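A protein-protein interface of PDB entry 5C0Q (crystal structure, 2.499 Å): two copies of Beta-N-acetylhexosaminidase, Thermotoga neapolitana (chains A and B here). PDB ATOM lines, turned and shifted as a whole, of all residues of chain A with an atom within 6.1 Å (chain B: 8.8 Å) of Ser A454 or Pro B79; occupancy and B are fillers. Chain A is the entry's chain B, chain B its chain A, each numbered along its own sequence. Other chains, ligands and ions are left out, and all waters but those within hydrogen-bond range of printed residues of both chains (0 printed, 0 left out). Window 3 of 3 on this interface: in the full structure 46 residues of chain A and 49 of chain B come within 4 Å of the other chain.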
ATOM      1  N   ILE A 325     -15.283  10.438  23.114  1.00  0.00           N
ATOM      2  CA  ILE A 325     -14.880   9.563  24.182  1.00  0.00           C
ATOM      3  C   ILE A 325     -16.075   9.077  24.955  1.00  0.00           C
ATOM      4  O   ILE A 325     -16.146   7.904  25.322  1.00  0.00           O
ATOM      5  CB  ILE A 325     -13.904  10.258  25.106  1.00  0.00           C
ATOM      6  CG1 ILE A 325     -12.609  10.496  24.347  1.00  0.00           C
ATOM      7  CG2 ILE A 325     -13.679   9.454  26.385  1.00  0.00           C
ATOM      8  CD1 ILE A 325     -11.659  11.377  25.035  1.00  0.00           C
ATOM      9  N   VAL A 328     -17.766   6.312  22.845  1.00  0.00           N
ATOM     10  CA  VAL A 328     -17.077   5.049  22.897  1.00  0.00           C
ATOM     11  C   VAL A 328     -17.507   4.328  24.169  1.00  0.00           C
ATOM     12  O   VAL A 328     -17.846   3.145  24.122  1.00  0.00           O
ATOM     13  CB  VAL A 328     -15.547   5.225  22.834  1.00  0.00           C
ATOM     14  CG1 VAL A 328     -14.859   3.990  23.175  1.00  0.00           C
ATOM     15  CG2 VAL A 328     -15.138   5.674  21.479  1.00  0.00           C
ATOM     16  N   ALA A 329     -17.498   5.052  25.286  1.00  0.00           N
ATOM     17  CA  ALA A 329     -17.861   4.497  26.570  1.00  0.00           C
ATOM     18  C   ALA A 329     -19.298   4.038  26.584  1.00  0.00           C
ATOM     19  O   ALA A 329     -19.583   2.951  27.008  1.00  0.00           O
ATOM     20  CB  ALA A 329     -17.630   5.490  27.639  1.00  0.00           C
ATOM     21  N   GLU A 330     -20.190   4.852  26.055  1.00  0.00           N
ATOM     22  CA  GLU A 330     -21.593   4.501  25.974  1.00  0.00           C
ATOM     23  C   GLU A 330     -21.817   3.212  25.159  1.00  0.00           C
ATOM     24  O   GLU A 330     -22.547   2.318  25.557  1.00  0.00           O
ATOM     25  CB  GLU A 330     -22.357   5.660  25.361  1.00  0.00           C
ATOM     26  CG  GLU A 330     -23.877   5.529  25.304  1.00  0.00           C
ATOM     27  CD  GLU A 330     -24.533   6.616  24.438  1.00  0.00           C
ATOM     28  OE1 GLU A 330     -24.834   7.729  24.953  1.00  0.00           O
ATOM     29  OE2 GLU A 330     -24.714   6.355  23.218  1.00  0.00           O
ATOM     30  N   ALA A 332     -19.772   0.776  24.352  1.00  0.00           N
ATOM     31  CA  ALA A 332     -19.067  -0.408  24.788  1.00  0.00           C
ATOM     32  C   ALA A 332     -19.731  -1.075  25.974  1.00  0.00           C
ATOM     33  O   ALA A 332     -19.163  -1.982  26.580  1.00  0.00           O
ATOM     34  CB  ALA A 332     -17.656  -0.078  25.146  1.00  0.00           C
ATOM     35  N   ILE A 333     -20.946  -0.673  26.289  1.00  0.00           N
ATOM     36  CA  ILE A 333     -21.627  -1.239  27.428  1.00  0.00           C
ATOM     37  C   ILE A 333     -22.639  -2.293  26.996  1.00  0.00           C
ATOM     38  O   ILE A 333     -23.469  -2.045  26.140  1.00  0.00           O
ATOM     39  CB  ILE A 333     -22.275  -0.128  28.252  1.00  0.00           C
ATOM     40  CG1 ILE A 333     -21.172   0.482  29.114  1.00  0.00           C
ATOM     41  CG2 ILE A 333     -23.368  -0.674  29.154  1.00  0.00           C
ATOM     42  CD1 ILE A 333     -21.454   1.734  29.545  1.00  0.00           C
ATOM     43  N   THR A 447     -18.638  -3.331  31.164  1.00  0.00           N
ATOM     44  CA  THR A 447     -18.235  -1.999  30.773  1.00  0.00           C
ATOM     45  C   THR A 447     -17.065  -1.984  29.837  1.00  0.00           C
ATOM     46  O   THR A 447     -16.875  -1.028  29.120  1.00  0.00           O
ATOM     47  CB  THR A 447     -17.848  -1.157  31.963  1.00  0.00           C
ATOM     48  OG1 THR A 447     -16.950  -1.920  32.771  1.00  0.00           O
ATOM     49  CG2 THR A 447     -19.056  -0.772  32.762  1.00  0.00           C
ATOM     50  N   HIS A 448     -16.239  -3.013  29.919  1.00  0.00           N
ATOM     51  CA  HIS A 448     -15.009  -3.105  29.152  1.00  0.00           C
ATOM     52  C   HIS A 448     -14.006  -2.050  29.568  1.00  0.00           C
ATOM     53  O   HIS A 448     -13.045  -1.821  28.858  1.00  0.00           O
ATOM     54  CB  HIS A 448     -15.261  -2.989  27.642  1.00  0.00           C
ATOM     55  CG  HIS A 448     -16.191  -4.020  27.095  1.00  0.00           C
ATOM     56  ND1 HIS A 448     -17.493  -3.738  26.748  1.00  0.00           N
ATOM     57  CD2 HIS A 448     -16.014  -5.339  26.856  1.00  0.00           C
ATOM     58  CE1 HIS A 448     -18.067  -4.835  26.293  1.00  0.00           C
ATOM     59  NE2 HIS A 448     -17.190  -5.817  26.342  1.00  0.00           N
ATOM     60  N   SER A 449     -14.229  -1.424  30.721  1.00  0.00           N
ATOM     61  CA  SER A 449     -13.353  -0.358  31.199  1.00  0.00           C
ATOM     62  C   SER A 449     -13.546  -0.025  32.670  1.00  0.00           C
ATOM     63  O   SER A 449     -14.622  -0.145  33.192  1.00  0.00           O
ATOM     64  CB  SER A 449     -13.590   0.897  30.362  1.00  0.00           C
ATOM     65  OG  SER A 449     -12.788   1.961  30.785  1.00  0.00           O
ATOM     66  N   THR A 450     -12.489   0.406  33.327  1.00  0.00           N
ATOM     67  CA  THR A 450     -12.593   0.909  34.684  1.00  0.00           C
ATOM     68  C   THR A 450     -12.809   2.437  34.775  1.00  0.00           C
ATOM     69  O   THR A 450     -12.926   2.979  35.860  1.00  0.00           O
ATOM     70  CB  THR A 450     -11.345   0.580  35.478  1.00  0.00           C
ATOM     71  OG1 THR A 450     -10.224   1.161  34.814  1.00  0.00           O
ATOM     72  CG2 THR A 450     -11.137  -0.914  35.558  1.00  0.00           C
ATOM     73  N   LYS A 451     -12.869   3.124  33.653  1.00  0.00           N
ATOM     74  CA  LYS A 451     -12.859   4.568  33.674  1.00  0.00           C
ATOM     75  C   LYS A 451     -14.168   5.179  34.145  1.00  0.00           C
ATOM     76  O   LYS A 451     -15.245   4.681  33.822  1.00  0.00           O
ATOM     77  CB  LYS A 451     -12.527   5.120  32.289  1.00  0.00           C
ATOM     78  CG  LYS A 451     -11.185   4.716  31.784  1.00  0.00           C
ATOM     79  CD  LYS A 451     -10.095   5.181  32.644  1.00  0.00           C
ATOM     80  CE  LYS A 451      -8.826   5.030  31.915  1.00  0.00           C
ATOM     81  NZ  LYS A 451      -7.643   5.224  32.746  1.00  0.00           N
ATOM     82  N   PRO A 452     -14.066   6.266  34.914  1.00  0.00           N
ATOM     83  CA  PRO A 452     -15.252   6.946  35.429  1.00  0.00           C
ATOM     84  C   PRO A 452     -16.322   7.198  34.373  1.00  0.00           C
ATOM     85  O   PRO A 452     -17.470   6.953  34.678  1.00  0.00           O
ATOM     86  CB  PRO A 452     -14.680   8.260  35.965  1.00  0.00           C
ATOM     87  CG  PRO A 452     -13.327   7.941  36.369  1.00  0.00           C
ATOM     88  CD  PRO A 452     -12.823   6.855  35.440  1.00  0.00           C
ATOM     89  N   ILE A 453     -15.971   7.589  33.157  1.00  0.00           N
ATOM     90  CA  ILE A 453     -16.976   7.798  32.124  1.00  0.00           C
ATOM     91  C   ILE A 453     -17.754   6.527  31.724  1.00  0.00           C
ATOM     92  O   ILE A 453     -18.954   6.606  31.401  1.00  0.00           O
ATOM     93  CB  ILE A 453     -16.343   8.460  30.877  1.00  0.00           C
ATOM     94  CG1 ILE A 453     -17.385   8.804  29.820  1.00  0.00           C
ATOM     95  CG2 ILE A 453     -15.270   7.584  30.269  1.00  0.00           C
ATOM     96  CD1 ILE A 453     -18.520   9.665  30.269  1.00  0.00           C
ATOM     97  N   SER A 454     -17.088   5.367  31.778  1.00  0.00           N
ATOM     98  CA  SER A 454     -17.704   4.074  31.460  1.00  0.00           C
ATOM     99  C   SER A 454     -18.680   3.653  32.572  1.00  0.00           C
ATOM    100  O   SER A 454     -19.809   3.224  32.322  1.00  0.00           O
ATOM    101  CB  SER A 454     -16.645   2.980  31.257  1.00  0.00           C
ATOM    102  OG  SER A 454     -16.009   3.046  30.003  1.00  0.00           O
ATOM    103  N   VAL A 455     -18.201   3.758  33.801  1.00  0.00           N
ATOM    104  CA  VAL A 455     -19.002   3.480  34.964  1.00  0.00           C
ATOM    105  C   VAL A 455     -20.233   4.364  34.921  1.00  0.00           C
ATOM    106  O   VAL A 455     -21.345   3.913  35.112  1.00  0.00           O
ATOM    107  CB  VAL A 455     -18.209   3.715  36.246  1.00  0.00           C
ATOM    108  CG1 VAL A 455     -19.044   3.327  37.408  1.00  0.00           C
ATOM    109  CG2 VAL A 455     -16.990   2.849  36.263  1.00  0.00           C
ATOM    110  N   TYR A 456     -20.001   5.641  34.653  1.00  0.00           N
ATOM    111  CA  TYR A 456     -21.043   6.632  34.451  1.00  0.00           C
ATOM    112  C   TYR A 456     -22.017   6.224  33.360  1.00  0.00           C
ATOM    113  O   TYR A 456     -23.220   6.260  33.561  1.00  0.00           O
ATOM    114  CB  TYR A 456     -20.376   7.972  34.129  1.00  0.00           C
ATOM    115  CG  TYR A 456     -21.235   9.093  33.683  1.00  0.00           C
ATOM    116  CD1 TYR A 456     -21.715   9.156  32.383  1.00  0.00           C
ATOM    117  CD2 TYR A 456     -21.488  10.154  34.524  1.00  0.00           C
ATOM    118  CE1 TYR A 456     -22.473  10.190  31.965  1.00  0.00           C
ATOM    119  CE2 TYR A 456     -22.238  11.227  34.104  1.00  0.00           C
ATOM    120  CZ  TYR A 456     -22.721  11.245  32.832  1.00  0.00           C
ATOM    121  OH  TYR A 456     -23.445  12.311  32.438  1.00  0.00           O
ATOM    122  N   LYS A 457     -21.507   5.834  32.198  1.00  0.00           N
ATOM    123  CA  LYS A 457     -22.410   5.441  31.133  1.00  0.00           C
ATOM    124  C   LYS A 457     -23.121   4.121  31.477  1.00  0.00           C
ATOM    125  O   LYS A 457     -24.222   3.850  31.005  1.00  0.00           O
ATOM    126  CB  LYS A 457     -21.664   5.294  29.806  1.00  0.00           C
ATOM    127  CG  LYS A 457     -21.295   6.598  29.154  1.00  0.00           C
ATOM    128  CD  LYS A 457     -22.535   7.327  28.812  1.00  0.00           C
ATOM    129  CE  LYS A 457     -22.283   8.663  28.184  1.00  0.00           C
ATOM    130  NZ  LYS A 457     -23.593   9.168  27.871  1.00  0.00           N
ATOM    131  N   SER A 458     -22.500   3.299  32.317  1.00  0.00           N
ATOM    132  CA  SER A 458     -23.140   2.054  32.697  1.00  0.00           C
ATOM    133  C   SER A 458     -24.360   2.349  33.591  1.00  0.00           C
ATOM    134  O   SER A 458     -25.403   1.732  33.427  1.00  0.00           O
ATOM    135  CB  SER A 458     -22.137   1.101  33.366  1.00  0.00           C
ATOM    136  OG  SER A 458     -22.032   1.279  34.755  1.00  0.00           O
ATOM    137  N   PHE A 459     -24.256   3.323  34.481  1.00  0.00           N
ATOM    138  CA  PHE A 459     -25.437   3.763  35.248  1.00  0.00           C
ATOM    139  C   PHE A 459     -26.531   4.360  34.353  1.00  0.00           C
ATOM    140  O   PHE A 459     -27.716   4.130  34.572  1.00  0.00           O
ATOM    141  CB  PHE A 459     -25.028   4.763  36.316  1.00  0.00           C
ATOM    142  CG  PHE A 459     -24.087   4.207  37.306  1.00  0.00           C
ATOM    143  CD1 PHE A 459     -24.200   2.914  37.722  1.00  0.00           C
ATOM    144  CD2 PHE A 459     -23.034   4.945  37.762  1.00  0.00           C
ATOM    145  CE1 PHE A 459     -23.321   2.382  38.611  1.00  0.00           C
ATOM    146  CE2 PHE A 459     -22.155   4.412  38.655  1.00  0.00           C
ATOM    147  CZ  PHE A 459     -22.304   3.112  39.069  1.00  0.00           C
ATOM    148  N   GLU B  65      -1.039   5.360  25.752  1.00  0.00           N
ATOM    149  CA  GLU B  65      -1.841   4.454  24.922  1.00  0.00           C
ATOM    150  C   GLU B  65      -3.290   4.801  24.979  1.00  0.00           C
ATOM    151  O   GLU B  65      -4.057   4.426  24.111  1.00  0.00           O
ATOM    152  CB  GLU B  65      -1.691   2.984  25.366  1.00  0.00           C
ATOM    153  CG  GLU B  65      -0.301   2.420  25.332  1.00  0.00           C
ATOM    154  CD  GLU B  65      -0.201   0.953  25.842  1.00  0.00           C
ATOM    155  OE1 GLU B  65      -1.242   0.321  26.123  1.00  0.00           O
ATOM    156  OE2 GLU B  65       0.943   0.439  25.938  1.00  0.00           O
ATOM    157  N   GLY B  66      -3.661   5.503  26.040  1.00  0.00           N
ATOM    158  CA  GLY B  66      -5.049   5.638  26.412  1.00  0.00           C
ATOM    159  C   GLY B  66      -5.445   4.458  27.271  1.00  0.00           C
ATOM    160  O   GLY B  66      -4.788   3.440  27.264  1.00  0.00           O
ATOM    161  N   GLY B  67      -6.523   4.601  28.015  1.00  0.00           N
ATOM    162  CA  GLY B  67      -7.013   3.535  28.854  1.00  0.00           C
ATOM    163  C   GLY B  67      -6.118   3.249  30.026  1.00  0.00           C
ATOM    164  O   GLY B  67      -5.775   4.140  30.776  1.00  0.00           O
ATOM    165  N   GLN B  68      -5.694   2.004  30.147  1.00  0.00           N
ATOM    166  CA  GLN B  68      -5.003   1.583  31.336  1.00  0.00           C
ATOM    167  C   GLN B  68      -3.675   2.288  31.478  1.00  0.00           C
ATOM    168  O   GLN B  68      -3.299   2.675  32.559  1.00  0.00           O
ATOM    169  CB  GLN B  68      -4.783   0.080  31.316  1.00  0.00           C
ATOM    170  CG  GLN B  68      -4.420  -0.474  32.638  1.00  0.00           C
ATOM    171  CD  GLN B  68      -4.218  -1.960  32.597  1.00  0.00           C
ATOM    172  OE1 GLN B  68      -4.849  -2.673  31.810  1.00  0.00           O
ATOM    173  NE2 GLN B  68      -3.374  -2.454  33.495  1.00  0.00           N
ATOM    174  N   LEU B  69      -2.995   2.521  30.376  1.00  0.00           N
ATOM    175  CA  LEU B  69      -1.733   3.222  30.422  1.00  0.00           C
ATOM    176  C   LEU B  69      -1.854   4.684  29.975  1.00  0.00           C
ATOM    177  O   LEU B  69      -1.845   4.971  28.788  1.00  0.00           O
ATOM    178  CB  LEU B  69      -0.740   2.502  29.531  1.00  0.00           C
ATOM    179  CG  LEU B  69       0.651   2.411  30.115  1.00  0.00           C
ATOM    180  CD1 LEU B  69       0.574   1.508  31.359  1.00  0.00           C
ATOM    181  CD2 LEU B  69       1.609   1.866  29.096  1.00  0.00           C
ATOM    182  N   GLU B  70      -1.974   5.606  30.924  1.00  0.00           N
ATOM    183  CA  GLU B  70      -2.060   7.022  30.609  1.00  0.00           C
ATOM    184  C   GLU B  70      -1.044   7.843  31.377  1.00  0.00           C
ATOM    185  O   GLU B  70      -0.916   7.729  32.578  1.00  0.00           O
ATOM    186  CB  GLU B  70      -3.476   7.522  30.847  1.00  0.00           C
ATOM    187  CG  GLU B  70      -4.378   7.094  29.748  1.00  0.00           C
ATOM    188  CD  GLU B  70      -5.818   7.454  29.934  1.00  0.00           C
ATOM    189  OE1 GLU B  70      -6.273   7.689  31.062  1.00  0.00           O
ATOM    190  OE2 GLU B  70      -6.521   7.480  28.922  1.00  0.00           O
ATOM    191  N   PRO B  76      -7.291  13.973  27.181  1.00  0.00           N
ATOM    192  CA  PRO B  76      -8.415  13.423  27.928  1.00  0.00           C
ATOM    193  C   PRO B  76      -8.362  11.904  27.997  1.00  0.00           C
ATOM    194  O   PRO B  76      -8.000  11.264  27.032  1.00  0.00           O
ATOM    195  CB  PRO B  76      -9.624  13.862  27.124  1.00  0.00           C
ATOM    196  CG  PRO B  76      -9.160  14.906  26.323  1.00  0.00           C
ATOM    197  CD  PRO B  76      -7.735  14.721  26.018  1.00  0.00           C
ATOM    198  N   SER B  77      -8.796  11.367  29.122  1.00  0.00           N
ATOM    199  CA  SER B  77      -8.741   9.961  29.435  1.00  0.00           C
ATOM    200  C   SER B  77      -9.735   9.145  28.582  1.00  0.00           C
ATOM    201  O   SER B  77     -10.859   9.569  28.348  1.00  0.00           O
ATOM    202  CB  SER B  77      -9.004   9.781  30.931  1.00  0.00           C
ATOM    203  OG  SER B  77      -8.881   8.454  31.329  1.00  0.00           O
ATOM    204  N   PHE B  78      -9.298   7.959  28.169  1.00  0.00           N
ATOM    205  CA  PHE B  78      -9.994   7.114  27.205  1.00  0.00           C
ATOM    206  C   PHE B  78     -10.289   5.780  27.870  1.00  0.00           C
ATOM    207  O   PHE B  78      -9.493   5.302  28.657  1.00  0.00           O
ATOM    208  CB  PHE B  78      -9.113   6.936  25.965  1.00  0.00           C
ATOM    209  CG  PHE B  78      -9.829   6.395  24.758  1.00  0.00           C
ATOM    210  CD1 PHE B  78     -10.907   7.070  24.228  1.00  0.00           C
ATOM    211  CD2 PHE B  78      -9.397   5.227  24.146  1.00  0.00           C
ATOM    212  CE1 PHE B  78     -11.540   6.594  23.146  1.00  0.00           C
ATOM    213  CE2 PHE B  78     -10.057   4.724  23.067  1.00  0.00           C
ATOM    214  CZ  PHE B  78     -11.119   5.400  22.557  1.00  0.00           C
ATOM    215  N   PRO B  79     -11.469   5.213  27.635  1.00  0.00           N
ATOM    216  CA  PRO B  79     -11.771   3.894  28.203  1.00  0.00           C
ATOM    217  C   PRO B  79     -10.712   2.851  27.855  1.00  0.00           C
ATOM    218  O   PRO B  79     -10.434   1.998  28.667  1.00  0.00           O
ATOM    219  CB  PRO B  79     -13.120   3.542  27.589  1.00  0.00           C
ATOM    220  CG  PRO B  79     -13.744   4.777  27.307  1.00  0.00           C
ATOM    221  CD  PRO B  79     -12.641   5.773  26.951  1.00  0.00           C
ATOM    222  N   GLY B  80     -10.119   2.936  26.676  1.00  0.00           N
ATOM    223  CA  GLY B  80      -9.055   2.035  26.324  1.00  0.00           C
ATOM    224  C   GLY B  80      -9.430   1.170  25.139  1.00  0.00           C
ATOM    225  O   GLY B  80     -10.550   1.215  24.634  1.00  0.00           O
ATOM    226  N   ASN B  81      -8.476   0.371  24.704  1.00  0.00           N
ATOM    227  CA  ASN B  81      -8.631  -0.470  23.516  1.00  0.00           C
ATOM    228  C   ASN B  81      -9.744  -1.531  23.617  1.00  0.00           C
ATOM    229  O   ASN B  81     -10.483  -1.743  22.666  1.00  0.00           O
ATOM    230  CB  ASN B  81      -7.311  -1.127  23.198  1.00  0.00           C
ATOM    231  CG  ASN B  81      -6.370  -0.222  22.434  1.00  0.00           C
ATOM    232  OD1 ASN B  81      -6.584   0.953  22.301  1.00  0.00           O
ATOM    233  ND2 ASN B  81      -5.311  -0.800  21.925  1.00  0.00           N
ATOM    234  N   LEU B  82      -9.895  -2.160  24.776  1.00  0.00           N
ATOM    235  CA  LEU B  82     -10.910  -3.188  24.881  1.00  0.00           C
ATOM    236  C   LEU B  82     -12.285  -2.588  24.628  1.00  0.00           C
ATOM    237  O   LEU B  82     -13.061  -3.126  23.876  1.00  0.00           O
ATOM    238  CB  LEU B  82     -10.871  -3.897  26.230  1.00  0.00           C
ATOM    239  CG  LEU B  82     -11.892  -5.039  26.269  1.00  0.00           C
ATOM    240  CD1 LEU B  82     -11.391  -6.227  25.513  1.00  0.00           C
ATOM    241  CD2 LEU B  82     -12.230  -5.426  27.687  1.00  0.00           C
ATOM    242  N   ALA B  83     -12.552  -1.429  25.194  1.00  0.00           N
ATOM    243  CA  ALA B  83     -13.793  -0.745  24.929  1.00  0.00           C
ATOM    244  C   ALA B  83     -13.883  -0.271  23.475  1.00  0.00           C
ATOM    245  O   ALA B  83     -14.932  -0.359  22.863  1.00  0.00           O
ATOM    246  CB  ALA B  83     -13.952   0.400  25.894  1.00  0.00           C
ATOM    247  N   ALA B  84     -12.794   0.247  22.930  1.00  0.00           N
ATOM    248  CA  ALA B  84     -12.786   0.699  21.549  1.00  0.00           C
ATOM    249  C   ALA B  84     -13.140  -0.402  20.544  1.00  0.00           C
ATOM    250  O   ALA B  84     -13.870  -0.161  19.605  1.00  0.00           O
ATOM    251  CB  ALA B  84     -11.455   1.270  21.213  1.00  0.00           C
ATOM    252  N   GLY B  85     -12.595  -1.603  20.761  1.00  0.00           N
ATOM    253  CA  GLY B  85     -12.870  -2.790  19.967  1.00  0.00           C
ATOM    254  C   GLY B  85     -14.346  -3.098  19.821  1.00  0.00           C
ATOM    255  O   GLY B  85     -14.754  -3.613  18.813  1.00  0.00           O
ATOM    256  N   VAL B  87     -16.514  -1.014  19.346  1.00  0.00           N
ATOM    257  CA  VAL B  87     -17.165   0.109  18.720  1.00  0.00           C
ATOM    258  C   VAL B  87     -16.701   0.303  17.296  1.00  0.00           C
ATOM    259  O   VAL B  87     -15.641  -0.134  16.952  1.00  0.00           O
ATOM    260  CB  VAL B  87     -16.928   1.381  19.629  1.00  0.00           C
ATOM    261  CG1 VAL B  87     -17.301   2.657  18.968  1.00  0.00           C
ATOM    262  CG2 VAL B  87     -17.695   1.224  20.916  1.00  0.00           C
ATOM    263  N   TYR B  95     -10.182   9.275  18.201  1.00  0.00           N
ATOM    264  CA  TYR B  95      -9.535   9.434  19.480  1.00  0.00           C
ATOM    265  C   TYR B  95      -8.065   9.749  19.295  1.00  0.00           C
ATOM    266  O   TYR B  95      -7.546  10.717  19.853  1.00  0.00           O
ATOM    267  CB  TYR B  95      -9.725   8.192  20.362  1.00  0.00           C
ATOM    268  CG  TYR B  95      -8.699   8.159  21.438  1.00  0.00           C
ATOM    269  CD1 TYR B  95      -8.689   9.143  22.433  1.00  0.00           C
ATOM    270  CD2 TYR B  95      -7.713   7.194  21.460  1.00  0.00           C
ATOM    271  CE1 TYR B  95      -7.735   9.170  23.398  1.00  0.00           C
ATOM    272  CE2 TYR B  95      -6.765   7.210  22.444  1.00  0.00           C
ATOM    273  CZ  TYR B  95      -6.798   8.215  23.425  1.00  0.00           C
ATOM    274  OH  TYR B  95      -5.864   8.265  24.405  1.00  0.00           O
ATOM    275  N   LEU B 129      -6.956  -5.090  29.220  1.00  0.00           N
ATOM    276  CA  LEU B 129      -7.656  -3.928  28.655  1.00  0.00           C
ATOM    277  C   LEU B 129      -6.943  -3.185  27.525  1.00  0.00           C
ATOM    278  O   LEU B 129      -7.589  -2.443  26.797  1.00  0.00           O
ATOM    279  CB  LEU B 129      -7.954  -2.904  29.734  1.00  0.00           C
ATOM    280  CG  LEU B 129      -9.059  -3.066  30.761  1.00  0.00           C
ATOM    281  CD1 LEU B 129      -9.127  -1.801  31.475  1.00  0.00           C
ATOM    282  CD2 LEU B 129     -10.400  -3.380  30.164  1.00  0.00           C
ATOM    283  N   ARG B 130      -5.663  -3.467  27.319  1.00  0.00           N
ATOM    284  CA  ARG B 130      -4.842  -2.733  26.395  1.00  0.00           C
ATOM    285  C   ARG B 130      -4.968  -3.231  24.947  1.00  0.00           C
ATOM    286  O   ARG B 130      -4.435  -2.625  24.016  1.00  0.00           O
ATOM    287  CB  ARG B 130      -3.386  -2.765  26.869  1.00  0.00           C
ATOM    288  CG  ARG B 130      -3.159  -1.933  28.139  1.00  0.00           C
ATOM    289  CD  ARG B 130      -1.819  -2.140  28.820  1.00  0.00           C
ATOM    290  NE  ARG B 130      -0.697  -1.847  27.935  1.00  0.00           N
ATOM    291  CZ  ARG B 130       0.565  -2.232  28.130  1.00  0.00           C
ATOM    292  NH1 ARG B 130       0.904  -2.901  29.213  1.00  0.00           N
ATOM    293  NH2 ARG B 130       1.508  -1.914  27.260  1.00  0.00           N
ATOM    294  N   SER B 131      -5.730  -4.298  24.760  1.00  0.00           N
ATOM    295  CA  SER B 131      -5.927  -4.884  23.471  1.00  0.00           C
ATOM    296  C   SER B 131      -7.312  -4.600  22.935  1.00  0.00           C
ATOM    297  O   SER B 131      -8.255  -4.630  23.671  1.00  0.00           O
ATOM    298  CB  SER B 131      -5.659  -6.419  23.564  1.00  0.00           C
ATOM    299  OG  SER B 131      -6.304  -7.181  22.563  1.00  0.00           O
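Among the printed residues, merely in contact across the chains: His A448 with Leu B129, Lys A451 with Phe B78, Ile A325 with Ser B77, Lys A451 with Ser B77, Ala A332 with Ala B83, His A448 with Ala B83, Lys A451 with Pro B79, Val A328 with Val B87, Ser A454 with Pro B79, Ile A325 with Phe B78, Ile A325 with Pro B76, Ile A325 with Pro B79, His A448 with Leu B82 and Ala A329 with Pro B79.
No position is printed for both chains.
Of the 17 pairs that touch across the chains among the printed residues, none has its exchanged pair printed and touching as well.
The backbone NH of Gly B67 sits at hydrogen-bond distance from the side-chain carboxylate of Glu B70.
The backbone NH (N) of Phe B78 sits at hydrogen-bond distance from the side-chain carboxylate (OE2) of Glu B70, 2.9 Å away.
The backbone NH (N) of Leu B82 lies within hydrogen-bond range of the backbone carbonyl oxygen (O) of Leu B129 (3.1 Å).
The side-chain hydroxyl of Thr A447 sits at hydrogen-bond distance from the backbone carbonyl oxygen of Ser A449, 3.0 Å away.
The backbone carbonyl oxygen (O) of Ser B131 is in hydrogen-bond range of the backbone NH (N) of Leu B82 (3.2 Å).
The side-chain hydroxyl (OG) of Ser A449 is in hydrogen-bond range of the backbone NH (N) of Lys A451, at 3.1 Å.
Of the 19 printed residues of chain A, 8 touch a printed residue of chain B.
Hydrophobic or aromatic side chains of chain B that line the printed part of chain A: Pro B76, Phe B78, Pro B79, Leu B82, Ala B83, Val B87 and Leu B129.
Along chain B the printed residues that touch a printed residue of chain A span positions 67 to 129.
Among the printed residues, Asp or Glu carboxylates within 4 Å of a Lys or Arg side-chain nitrogen of the other chain: Lys A451 with Glu B70 (3.3 Å).
The side-chain amino group (NZ) of Lys A451 is in salt-bridge range of the side-chain carboxylate (OE1) of Glu B70 (3.3 Å).
The backbone carbonyl oxygen (O) of Pro B79 is in hydrogen-bond range of the side-chain hydroxyl (OG) of Ser A449, at 3.2 Å.
NZ of Lys A451 is in hydrogen-bond range of O of Gly B67 (2.9 Å).
Ser A454 touches one residue of chain B.
Of the printed residues of chain B, His A448 touches Leu B82, Ala B83 and Leu B129.
Of the printed residues of chain A, Phe B78 touches Ile A325 and Lys A451.
Of the printed residues of chain A, Ala B83 touches Ala A332 (3.6 Å) and His A448 (3.7 Å).
Printed residues of chain B within 4 Å of Val A328: Val B87 (3.7 Å).
Of the printed residues of chain B, Ile A325 touches Pro B76, Ser B77, Phe B78 and Pro B79.
The nearest printed residue of chain A that does not touch Pro B79 is Val A328 (4.4 Å).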
